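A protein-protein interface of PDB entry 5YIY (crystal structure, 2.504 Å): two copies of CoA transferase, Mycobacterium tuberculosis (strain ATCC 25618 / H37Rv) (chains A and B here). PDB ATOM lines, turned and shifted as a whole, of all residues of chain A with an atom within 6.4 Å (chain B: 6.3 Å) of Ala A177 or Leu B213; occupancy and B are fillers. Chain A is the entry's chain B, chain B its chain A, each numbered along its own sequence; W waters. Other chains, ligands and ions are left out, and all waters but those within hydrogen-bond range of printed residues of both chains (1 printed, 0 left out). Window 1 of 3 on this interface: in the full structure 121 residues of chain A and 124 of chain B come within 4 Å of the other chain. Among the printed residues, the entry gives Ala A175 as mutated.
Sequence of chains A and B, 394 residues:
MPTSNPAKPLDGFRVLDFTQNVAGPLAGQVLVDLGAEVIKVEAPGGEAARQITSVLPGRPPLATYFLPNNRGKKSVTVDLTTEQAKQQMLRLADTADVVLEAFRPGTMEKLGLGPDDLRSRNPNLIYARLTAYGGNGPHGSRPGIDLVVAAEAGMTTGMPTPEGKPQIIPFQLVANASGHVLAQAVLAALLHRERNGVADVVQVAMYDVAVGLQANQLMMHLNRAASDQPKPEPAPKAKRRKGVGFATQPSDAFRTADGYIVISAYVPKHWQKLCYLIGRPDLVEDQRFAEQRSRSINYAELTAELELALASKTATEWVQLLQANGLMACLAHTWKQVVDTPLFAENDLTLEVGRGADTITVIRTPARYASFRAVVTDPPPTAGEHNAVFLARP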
ATOM      1  N   LEU A  26     -18.924  20.756 -10.365  1.00  0.00           N
ATOM      2  CA  LEU A  26     -18.911  22.089  -9.768  1.00  0.00           C
ATOM      3  C   LEU A  26     -19.687  23.079 -10.629  1.00  0.00           C
ATOM      4  O   LEU A  26     -20.411  23.930 -10.111  1.00  0.00           O
ATOM      5  CB  LEU A  26     -17.476  22.582  -9.565  1.00  0.00           C
ATOM      6  CG  LEU A  26     -17.342  24.035  -9.100  1.00  0.00           C
ATOM      7  CD1 LEU A  26     -17.995  24.232  -7.740  1.00  0.00           C
ATOM      8  CD2 LEU A  26     -15.885  24.458  -9.062  1.00  0.00           C
ATOM      9  N   PHE A 171      -4.057  21.832  -3.631  1.00  0.00           N
ATOM     10  CA  PHE A 171      -5.503  21.911  -3.822  1.00  0.00           C
ATOM     11  C   PHE A 171      -5.859  21.917  -5.306  1.00  0.00           C
ATOM     12  O   PHE A 171      -5.013  22.187  -6.158  1.00  0.00           O
ATOM     13  CB  PHE A 171      -6.093  23.141  -3.120  1.00  0.00           C
ATOM     14  CG  PHE A 171      -5.424  24.439  -3.476  1.00  0.00           C
ATOM     15  CD1 PHE A 171      -4.344  24.902  -2.740  1.00  0.00           C
ATOM     16  CD2 PHE A 171      -5.889  25.208  -4.530  1.00  0.00           C
ATOM     17  CE1 PHE A 171      -3.733  26.103  -3.058  1.00  0.00           C
ATOM     18  CE2 PHE A 171      -5.281  26.408  -4.854  1.00  0.00           C
ATOM     19  CZ  PHE A 171      -4.202  26.856  -4.116  1.00  0.00           C
ATOM     20  N   GLN A 172      -7.119  21.615  -5.605  1.00  0.00           N
ATOM     21  CA  GLN A 172      -7.569  21.457  -6.983  1.00  0.00           C
ATOM     22  C   GLN A 172      -7.859  22.809  -7.627  1.00  0.00           C
ATOM     23  O   GLN A 172      -9.011  23.148  -7.899  1.00  0.00           O
ATOM     24  CB  GLN A 172      -8.813  20.564  -7.043  1.00  0.00           C
ATOM     25  CG  GLN A 172      -8.540  19.075  -6.841  1.00  0.00           C
ATOM     26  CD  GLN A 172      -8.019  18.751  -5.452  1.00  0.00           C
ATOM     27  OE1 GLN A 172      -8.644  19.089  -4.447  1.00  0.00           O
ATOM     28  NE2 GLN A 172      -6.867  18.091  -5.391  1.00  0.00           N
ATOM     29  N   LEU A 173      -6.800  23.573  -7.868  1.00  0.00           N
ATOM     30  CA  LEU A 173      -6.915  24.915  -8.426  1.00  0.00           C
ATOM     31  C   LEU A 173      -7.470  24.925  -9.848  1.00  0.00           C
ATOM     32  O   LEU A 173      -8.352  25.720 -10.170  1.00  0.00           O
ATOM     33  CB  LEU A 173      -5.548  25.602  -8.404  1.00  0.00           C
ATOM     34  CG  LEU A 173      -5.392  26.870  -9.244  1.00  0.00           C
ATOM     35  CD1 LEU A 173      -6.262  27.995  -8.702  1.00  0.00           C
ATOM     36  CD2 LEU A 173      -3.931  27.291  -9.305  1.00  0.00           C
ATOM     37  N   VAL A 174      -6.955  24.040 -10.694  1.00  0.00           N
ATOM     38  CA  VAL A 174      -7.355  24.004 -12.096  1.00  0.00           C
ATOM     39  C   VAL A 174      -8.786  23.499 -12.264  1.00  0.00           C
ATOM     40  O   VAL A 174      -9.565  24.064 -13.031  1.00  0.00           O
ATOM     41  CB  VAL A 174      -6.401  23.123 -12.926  1.00  0.00           C
ATOM     42  CG1 VAL A 174      -6.875  23.035 -14.368  1.00  0.00           C
ATOM     43  CG2 VAL A 174      -4.992  23.681 -12.867  1.00  0.00           C
ATOM     44  N   ALA A 175      -9.129  22.442 -11.534  1.00  0.00           N
ATOM     45  CA  ALA A 175     -10.452  21.836 -11.635  1.00  0.00           C
ATOM     46  C   ALA A 175     -11.541  22.791 -11.157  1.00  0.00           C
ATOM     47  O   ALA A 175     -12.585  22.922 -11.796  1.00  0.00           O
ATOM     48  CB  ALA A 175     -10.503  20.538 -10.843  1.00  0.00           C
ATOM     49  N   ASN A 176     -11.295  23.452 -10.031  1.00  0.00           N
ATOM     50  CA  ASN A 176     -12.258  24.397  -9.478  1.00  0.00           C
ATOM     51  C   ASN A 176     -12.415  25.633 -10.357  1.00  0.00           C
ATOM     52  O   ASN A 176     -13.520  26.149 -10.525  1.00  0.00           O
ATOM     53  CB  ASN A 176     -11.853  24.807  -8.061  1.00  0.00           C
ATOM     54  CG  ASN A 176     -12.134  23.721  -7.038  1.00  0.00           C
ATOM     55  OD1 ASN A 176     -13.077  22.942  -7.185  1.00  0.00           O
ATOM     56  ND2 ASN A 176     -11.315  23.665  -5.994  1.00  0.00           N
ATOM     57  N   ALA A 177     -11.306  26.107 -10.916  1.00  0.00           N
ATOM     58  CA  ALA A 177     -11.341  27.255 -11.814  1.00  0.00           C
ATOM     59  C   ALA A 177     -12.053  26.902 -13.115  1.00  0.00           C
ATOM     60  O   ALA A 177     -12.816  27.704 -13.652  1.00  0.00           O
ATOM     61  CB  ALA A 177      -9.934  27.757 -12.097  1.00  0.00           C
ATOM     62  N   SER A 178     -11.798  25.696 -13.614  1.00  0.00           N
ATOM     63  CA  SER A 178     -12.421  25.227 -14.847  1.00  0.00           C
ATOM     64  C   SER A 178     -13.931  25.100 -14.686  1.00  0.00           C
ATOM     65  O   SER A 178     -14.687  25.343 -15.627  1.00  0.00           O
ATOM     66  CB  SER A 178     -11.826  23.882 -15.274  1.00  0.00           C
ATOM     67  OG  SER A 178     -10.440  24.001 -15.542  1.00  0.00           O
ATOM     68  N   GLY A 179     -14.362  24.716 -13.488  1.00  0.00           N
ATOM     69  CA  GLY A 179     -15.776  24.584 -13.191  1.00  0.00           C
ATOM     70  C   GLY A 179     -16.515  25.903 -13.309  1.00  0.00           C
ATOM     71  O   GLY A 179     -17.611  25.965 -13.866  1.00  0.00           O
ATOM     72  N   HIS A 180     -15.909  26.962 -12.783  1.00  0.00           N
ATOM     73  CA  HIS A 180     -16.506  28.291 -12.841  1.00  0.00           C
ATOM     74  C   HIS A 180     -16.476  28.861 -14.255  1.00  0.00           C
ATOM     75  O   HIS A 180     -17.399  29.562 -14.668  1.00  0.00           O
ATOM     76  CB  HIS A 180     -15.795  29.237 -11.872  1.00  0.00           C
ATOM     77  CG  HIS A 180     -16.131  28.987 -10.435  1.00  0.00           C
ATOM     78  ND1 HIS A 180     -17.348  29.328  -9.886  1.00  0.00           N
ATOM     79  CD2 HIS A 180     -15.414  28.419  -9.436  1.00  0.00           C
ATOM     80  CE1 HIS A 180     -17.365  28.987  -8.611  1.00  0.00           C
ATOM     81  NE2 HIS A 180     -16.203  28.433  -8.313  1.00  0.00           N
ATOM     82  N   VAL A 181     -15.412  28.561 -14.994  1.00  0.00           N
ATOM     83  CA  VAL A 181     -15.304  28.996 -16.382  1.00  0.00           C
ATOM     84  C   VAL A 181     -16.350  28.292 -17.242  1.00  0.00           C
ATOM     85  O   VAL A 181     -16.974  28.908 -18.109  1.00  0.00           O
ATOM     86  CB  VAL A 181     -13.894  28.732 -16.953  1.00  0.00           C
ATOM     87  CG1 VAL A 181     -13.859  29.002 -18.450  1.00  0.00           C
ATOM     88  CG2 VAL A 181     -12.864  29.588 -16.233  1.00  0.00           C
ATOM     89  N   LEU A 182     -16.551  27.002 -16.989  1.00  0.00           N
ATOM     90  CA  LEU A 182     -17.547  26.228 -17.722  1.00  0.00           C
ATOM     91  C   LEU A 182     -18.955  26.731 -17.431  1.00  0.00           C
ATOM     92  O   LEU A 182     -19.775  26.860 -18.339  1.00  0.00           O
ATOM     93  CB  LEU A 182     -17.437  24.741 -17.377  1.00  0.00           C
ATOM     94  CG  LEU A 182     -18.486  23.831 -18.021  1.00  0.00           C
ATOM     95  CD1 LEU A 182     -18.356  23.848 -19.537  1.00  0.00           C
ATOM     96  CD2 LEU A 182     -18.368  22.412 -17.488  1.00  0.00           C
ATOM     97  N   VAL A 209      -7.671  26.767 -19.302  1.00  0.00           N
ATOM     98  CA  VAL A 209      -7.940  27.481 -18.061  1.00  0.00           C
ATOM     99  C   VAL A 209      -6.659  27.651 -17.249  1.00  0.00           C
ATOM    100  O   VAL A 209      -6.386  28.734 -16.730  1.00  0.00           O
ATOM    101  CB  VAL A 209      -8.998  26.757 -17.207  1.00  0.00           C
ATOM    102  CG1 VAL A 209      -9.160  27.444 -15.859  1.00  0.00           C
ATOM    103  CG2 VAL A 209     -10.328  26.707 -17.946  1.00  0.00           C
ATOM    104  N   LEU A 213      -4.722  31.137 -16.241  1.00  0.00           N
ATOM    105  CA  LEU A 213      -4.347  31.541 -14.889  1.00  0.00           C
ATOM    106  C   LEU A 213      -2.898  32.016 -14.812  1.00  0.00           C
ATOM    107  O   LEU A 213      -2.550  32.792 -13.913  1.00  0.00           O
ATOM    108  CB  LEU A 213      -4.589  30.393 -13.908  1.00  0.00           C
ATOM    109  CG  LEU A 213      -6.044  29.957 -13.714  1.00  0.00           C
ATOM    110  CD1 LEU A 213      -6.122  28.585 -13.063  1.00  0.00           C
ATOM    111  CD2 LEU A 213      -6.799  30.973 -12.873  1.00  0.00           C
ATOM    112  N   MET B 155      -3.501  29.704   1.109  1.00  0.00           N
ATOM    113  CA  MET B 155      -2.957  29.066  -0.088  1.00  0.00           C
ATOM    114  C   MET B 155      -1.476  28.693   0.011  1.00  0.00           C
ATOM    115  O   MET B 155      -0.944  28.031  -0.879  1.00  0.00           O
ATOM    116  CB  MET B 155      -3.174  29.964  -1.306  1.00  0.00           C
ATOM    117  CG  MET B 155      -4.592  29.922  -1.842  1.00  0.00           C
ATOM    118  SD  MET B 155      -4.800  30.808  -3.394  1.00  0.00           S
ATOM    119  CE  MET B 155      -6.456  30.297  -3.845  1.00  0.00           C
ATOM    120  N   LEU B 173      -3.331  33.649  -9.480  1.00  0.00           N
ATOM    121  CA  LEU B 173      -4.385  32.641  -9.546  1.00  0.00           C
ATOM    122  C   LEU B 173      -5.721  33.174  -9.023  1.00  0.00           C
ATOM    123  O   LEU B 173      -6.764  32.942  -9.632  1.00  0.00           O
ATOM    124  CB  LEU B 173      -3.977  31.376  -8.774  1.00  0.00           C
ATOM    125  CG  LEU B 173      -3.853  31.359  -7.245  1.00  0.00           C
ATOM    126  CD1 LEU B 173      -3.768  29.926  -6.748  1.00  0.00           C
ATOM    127  CD2 LEU B 173      -2.652  32.157  -6.757  1.00  0.00           C
ATOM    128  N   VAL B 174      -5.686  33.889  -7.903  1.00  0.00           N
ATOM    129  CA  VAL B 174      -6.905  34.386  -7.274  1.00  0.00           C
ATOM    130  C   VAL B 174      -7.562  35.482  -8.109  1.00  0.00           C
ATOM    131  O   VAL B 174      -8.778  35.484  -8.297  1.00  0.00           O
ATOM    132  CB  VAL B 174      -6.624  34.929  -5.857  1.00  0.00           C
ATOM    133  CG1 VAL B 174      -7.882  35.538  -5.253  1.00  0.00           C
ATOM    134  CG2 VAL B 174      -6.084  33.823  -4.970  1.00  0.00           C
ATOM    135  N   ALA B 177      -9.000  33.962 -11.384  1.00  0.00           N
ATOM    136  CA  ALA B 177     -10.169  33.143 -11.081  1.00  0.00           C
ATOM    137  C   ALA B 177     -11.356  34.015 -10.689  1.00  0.00           C
ATOM    138  O   ALA B 177     -12.490  33.745 -11.080  1.00  0.00           O
ATOM    139  CB  ALA B 177      -9.852  32.148  -9.974  1.00  0.00           C
ATOM    140  N   HIS B 180     -13.194  35.588 -13.723  1.00  0.00           N
ATOM    141  CA  HIS B 180     -14.123  34.690 -14.398  1.00  0.00           C
ATOM    142  C   HIS B 180     -15.385  34.477 -13.569  1.00  0.00           C
ATOM    143  O   HIS B 180     -16.480  34.348 -14.116  1.00  0.00           O
ATOM    144  CB  HIS B 180     -13.448  33.351 -14.697  1.00  0.00           C
ATOM    145  CG  HIS B 180     -12.455  33.413 -15.815  1.00  0.00           C
ATOM    146  ND1 HIS B 180     -12.830  33.521 -17.137  1.00  0.00           N
ATOM    147  CD2 HIS B 180     -11.101  33.391 -15.809  1.00  0.00           C
ATOM    148  CE1 HIS B 180     -11.751  33.558 -17.898  1.00  0.00           C
ATOM    149  NE2 HIS B 180     -10.688  33.482 -17.117  1.00  0.00           N
ATOM    150  N   ASP B 208     -13.440  34.946  -1.045  1.00  0.00           N
ATOM    151  CA  ASP B 208     -14.430  33.883  -1.191  1.00  0.00           C
ATOM    152  C   ASP B 208     -14.053  32.935  -2.323  1.00  0.00           C
ATOM    153  O   ASP B 208     -14.211  31.719  -2.205  1.00  0.00           O
ATOM    154  CB  ASP B 208     -15.819  34.474  -1.440  1.00  0.00           C
ATOM    155  CG  ASP B 208     -16.346  35.249  -0.249  1.00  0.00           C
ATOM    156  OD1 ASP B 208     -15.764  35.122   0.849  1.00  0.00           O
ATOM    157  OD2 ASP B 208     -17.343  35.985  -0.410  1.00  0.00           O
ATOM    158  N   VAL B 209     -13.553  33.499  -3.418  1.00  0.00           N
ATOM    159  CA  VAL B 209     -13.107  32.704  -4.555  1.00  0.00           C
ATOM    160  C   VAL B 209     -11.907  31.851  -4.164  1.00  0.00           C
ATOM    161  O   VAL B 209     -11.847  30.662  -4.482  1.00  0.00           O
ATOM    162  CB  VAL B 209     -12.737  33.595  -5.759  1.00  0.00           C
ATOM    163  CG1 VAL B 209     -12.143  32.757  -6.881  1.00  0.00           C
ATOM    164  CG2 VAL B 209     -13.957  34.360  -6.247  1.00  0.00           C
ATOM    165  N   ALA B 210     -10.959  32.466  -3.462  1.00  0.00           N
ATOM    166  CA  ALA B 210      -9.761  31.772  -3.007  1.00  0.00           C
ATOM    167  C   ALA B 210     -10.111  30.628  -2.059  1.00  0.00           C
ATOM    168  O   ALA B 210      -9.510  29.554  -2.118  1.00  0.00           O
ATOM    169  CB  ALA B 210      -8.811  32.747  -2.332  1.00  0.00           C
ATOM    170  N   VAL B 211     -11.086  30.867  -1.187  1.00  0.00           N
ATOM    171  CA  VAL B 211     -11.583  29.835  -0.285  1.00  0.00           C
ATOM    172  C   VAL B 211     -12.221  28.699  -1.081  1.00  0.00           C
ATOM    173  O   VAL B 211     -11.990  27.521  -0.801  1.00  0.00           O
ATOM    174  CB  VAL B 211     -12.606  30.409   0.722  1.00  0.00           C
ATOM    175  CG1 VAL B 211     -13.457  29.301   1.329  1.00  0.00           C
ATOM    176  CG2 VAL B 211     -11.892  31.201   1.810  1.00  0.00           C
ATOM    177  N   GLY B 212     -13.011  29.065  -2.086  1.00  0.00           N
ATOM    178  CA  GLY B 212     -13.673  28.095  -2.938  1.00  0.00           C
ATOM    179  C   GLY B 212     -12.701  27.230  -3.720  1.00  0.00           C
ATOM    180  O   GLY B 212     -12.981  26.065  -3.999  1.00  0.00           O
ATOM    181  N   LEU B 213     -11.553  27.802  -4.073  1.00  0.00           N
ATOM    182  CA  LEU B 213     -10.524  27.062  -4.796  1.00  0.00           C
ATOM    183  C   LEU B 213      -9.877  26.008  -3.902  1.00  0.00           C
ATOM    184  O   LEU B 213      -9.322  25.023  -4.390  1.00  0.00           O
ATOM    185  CB  LEU B 213      -9.459  28.016  -5.344  1.00  0.00           C
ATOM    186  CG  LEU B 213      -9.904  28.977  -6.448  1.00  0.00           C
ATOM    187  CD1 LEU B 213      -8.801  29.972  -6.774  1.00  0.00           C
ATOM    188  CD2 LEU B 213     -10.320  28.211  -7.693  1.00  0.00           C
ATOM    189  N   GLN B 214      -9.953  26.224  -2.592  1.00  0.00           N
ATOM    190  CA  GLN B 214      -9.396  25.290  -1.619  1.00  0.00           C
ATOM    191  C   GLN B 214     -10.500  24.578  -0.846  1.00  0.00           C
ATOM    192  O   GLN B 214     -10.266  24.073   0.254  1.00  0.00           O
ATOM    193  CB  GLN B 214      -8.477  26.018  -0.639  1.00  0.00           C
ATOM    194  CG  GLN B 214      -7.455  26.929  -1.284  1.00  0.00           C
ATOM    195  CD  GLN B 214      -6.738  27.791  -0.265  1.00  0.00           C
ATOM    196  OE1 GLN B 214      -5.734  27.380   0.317  1.00  0.00           O
ATOM    197  NE2 GLN B 214      -7.255  28.994  -0.040  1.00  0.00           N
ATOM    198  N   ALA B 215     -11.698  24.549  -1.425  1.00  0.00           N
ATOM    199  CA  ALA B 215     -12.883  24.022  -0.751  1.00  0.00           C
ATOM    200  C   ALA B 215     -12.681  22.605  -0.223  1.00  0.00           C
ATOM    201  O   ALA B 215     -13.065  22.301   0.903  1.00  0.00           O
ATOM    202  CB  ALA B 215     -14.079  24.063  -1.690  1.00  0.00           C
ATOM    203  N   ASN B 216     -12.074  21.748  -1.035  1.00  0.00           N
ATOM    204  CA  ASN B 216     -11.856  20.356  -0.655  1.00  0.00           C
ATOM    205  C   ASN B 216     -10.908  20.217   0.535  1.00  0.00           C
ATOM    206  O   ASN B 216     -11.042  19.298   1.343  1.00  0.00           O
ATOM    207  CB  ASN B 216     -11.314  19.564  -1.846  1.00  0.00           C
ATOM    208  CG  ASN B 216     -12.130  19.781  -3.107  1.00  0.00           C
ATOM    209  OD1 ASN B 216     -11.851  20.686  -3.893  1.00  0.00           O
ATOM    210  ND2 ASN B 216     -13.146  18.948  -3.305  1.00  0.00           N
ATOM    211  N   GLN B 217      -9.952  21.135   0.637  1.00  0.00           N
ATOM    212  CA  GLN B 217      -8.957  21.095   1.703  1.00  0.00           C
ATOM    213  C   GLN B 217      -9.495  21.688   3.002  1.00  0.00           C
ATOM    214  O   GLN B 217      -9.345  21.100   4.072  1.00  0.00           O
ATOM    215  CB  GLN B 217      -7.691  21.840   1.274  1.00  0.00           C
ATOM    216  CG  GLN B 217      -7.162  21.423  -0.087  1.00  0.00           C
ATOM    217  CD  GLN B 217      -6.750  19.965  -0.133  1.00  0.00           C
ATOM    218  OE1 GLN B 217      -6.280  19.409   0.859  1.00  0.00           O
ATOM    219  NE2 GLN B 217      -6.928  19.337  -1.291  1.00  0.00           N
HETATM  220  O   HOH W   1      -7.038  16.788  -2.271  1.00  0.00           O
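The backbone carbonyl oxygen (O) of Leu B213 sits at hydrogen-bond distance from the side-chain amide nitrogen (ND2) of Asn A176.
The backbone NH (N) of Met B155 sits close to the side-chain amide oxygen (OE1) of Gln B214 (3.3 Å).
The side-chain amide nitrogen (ND2) of Asn A176 sits at hydrogen-bond distance from the backbone carbonyl oxygen (O) of Gln A172, 3.0 Å away.
O of Ala B210 sits at hydrogen-bond distance from NE2 of Gln B214.
CZ of Phe A171 touches CG of Met B155, at 3.8 Å.
O of Gln A172 touches O of Leu B213 (3.99 Å).
Gln A172 touches Asn B216 (OE1 to OD1, 3.6 Å).
OE1 of Gln A172 touches NE2 of Gln B217, at 3.6 Å.
Leu B173 touches Leu A173 (CD1 to CD2, 3.7 Å).
OD1 of Asn B216 touches ND2 of Asn A176, at 3.7 Å.
Leu B213 touches Ala A177 (CD2 to N, 3.97 Å).
CG of His B180 touches CG2 of Val A181, at 3.9 Å.
CD2 of Leu A213 touches O of Leu B173 (3.8 Å).
Ala B177 touches Leu A213 (N to CD2, 3.999 Å).
Printed residues of chain B within 4 Å of Gln A172: Leu B213 (3.99 Å), Asn B216 (3.6 Å) and Gln B217 (3.6 Å).
Printed residues of chain B within 4 Å of Ala A177: Leu B213 (3.97 Å).
Leu A182 touches none of the printed residues of chain B.
Of the printed residues of chain A, Met B155 touches Phe A171.
Of the printed residues of chain A, Leu B173 touches Leu A173 and Leu A213.
Of the printed residues of chain A, Ala B177 touches Leu A213 (3.999 Å).
Of the printed residues of chain A, Leu B213 touches Phe A171 (3.4 Å), Gln A172 (3.99 Å), Leu A173 (3.8 Å), Asn A176 (2.9 Å) and Ala A177 (3.97 Å).
The nearest residue of chain B that does not touch Ala A177 is Ala B177 (4.9 Å).
Of the 15 printed residues of chain A, 7 touch a printed residue of chain B.
Printed residues of chain A that touch a printed residue of chain B: Phe A171, Gln A172, Leu A173, Asn A176, Ala A177, Val A181 and Leu A213.
Hydrophobic or aromatic side chains of chain A that line the printed part of chain B: Phe A171, Leu A173, Val A181 and Leu A213.
Among the printed residues, 16 pairs touch across the chains.
Among the printed residues, no Asp or Glu carboxylate lies within 4 Å of a Lys or Arg side-chain nitrogen of the other chain.
Leu B173 touches its own counterpart, Leu A173.
Leu A173 touches Leu B213, and with the chains exchanged Leu A213 touches Leu B173.
Ala A177 touches Leu B213, and with the chains exchanged Leu A213 touches Ala B177.
6 positions are printed for both chains.
Water W1 bridges NE2 of Gln B217 (2.7 Å) and NE2 of Gln A172 (3.4 Å).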
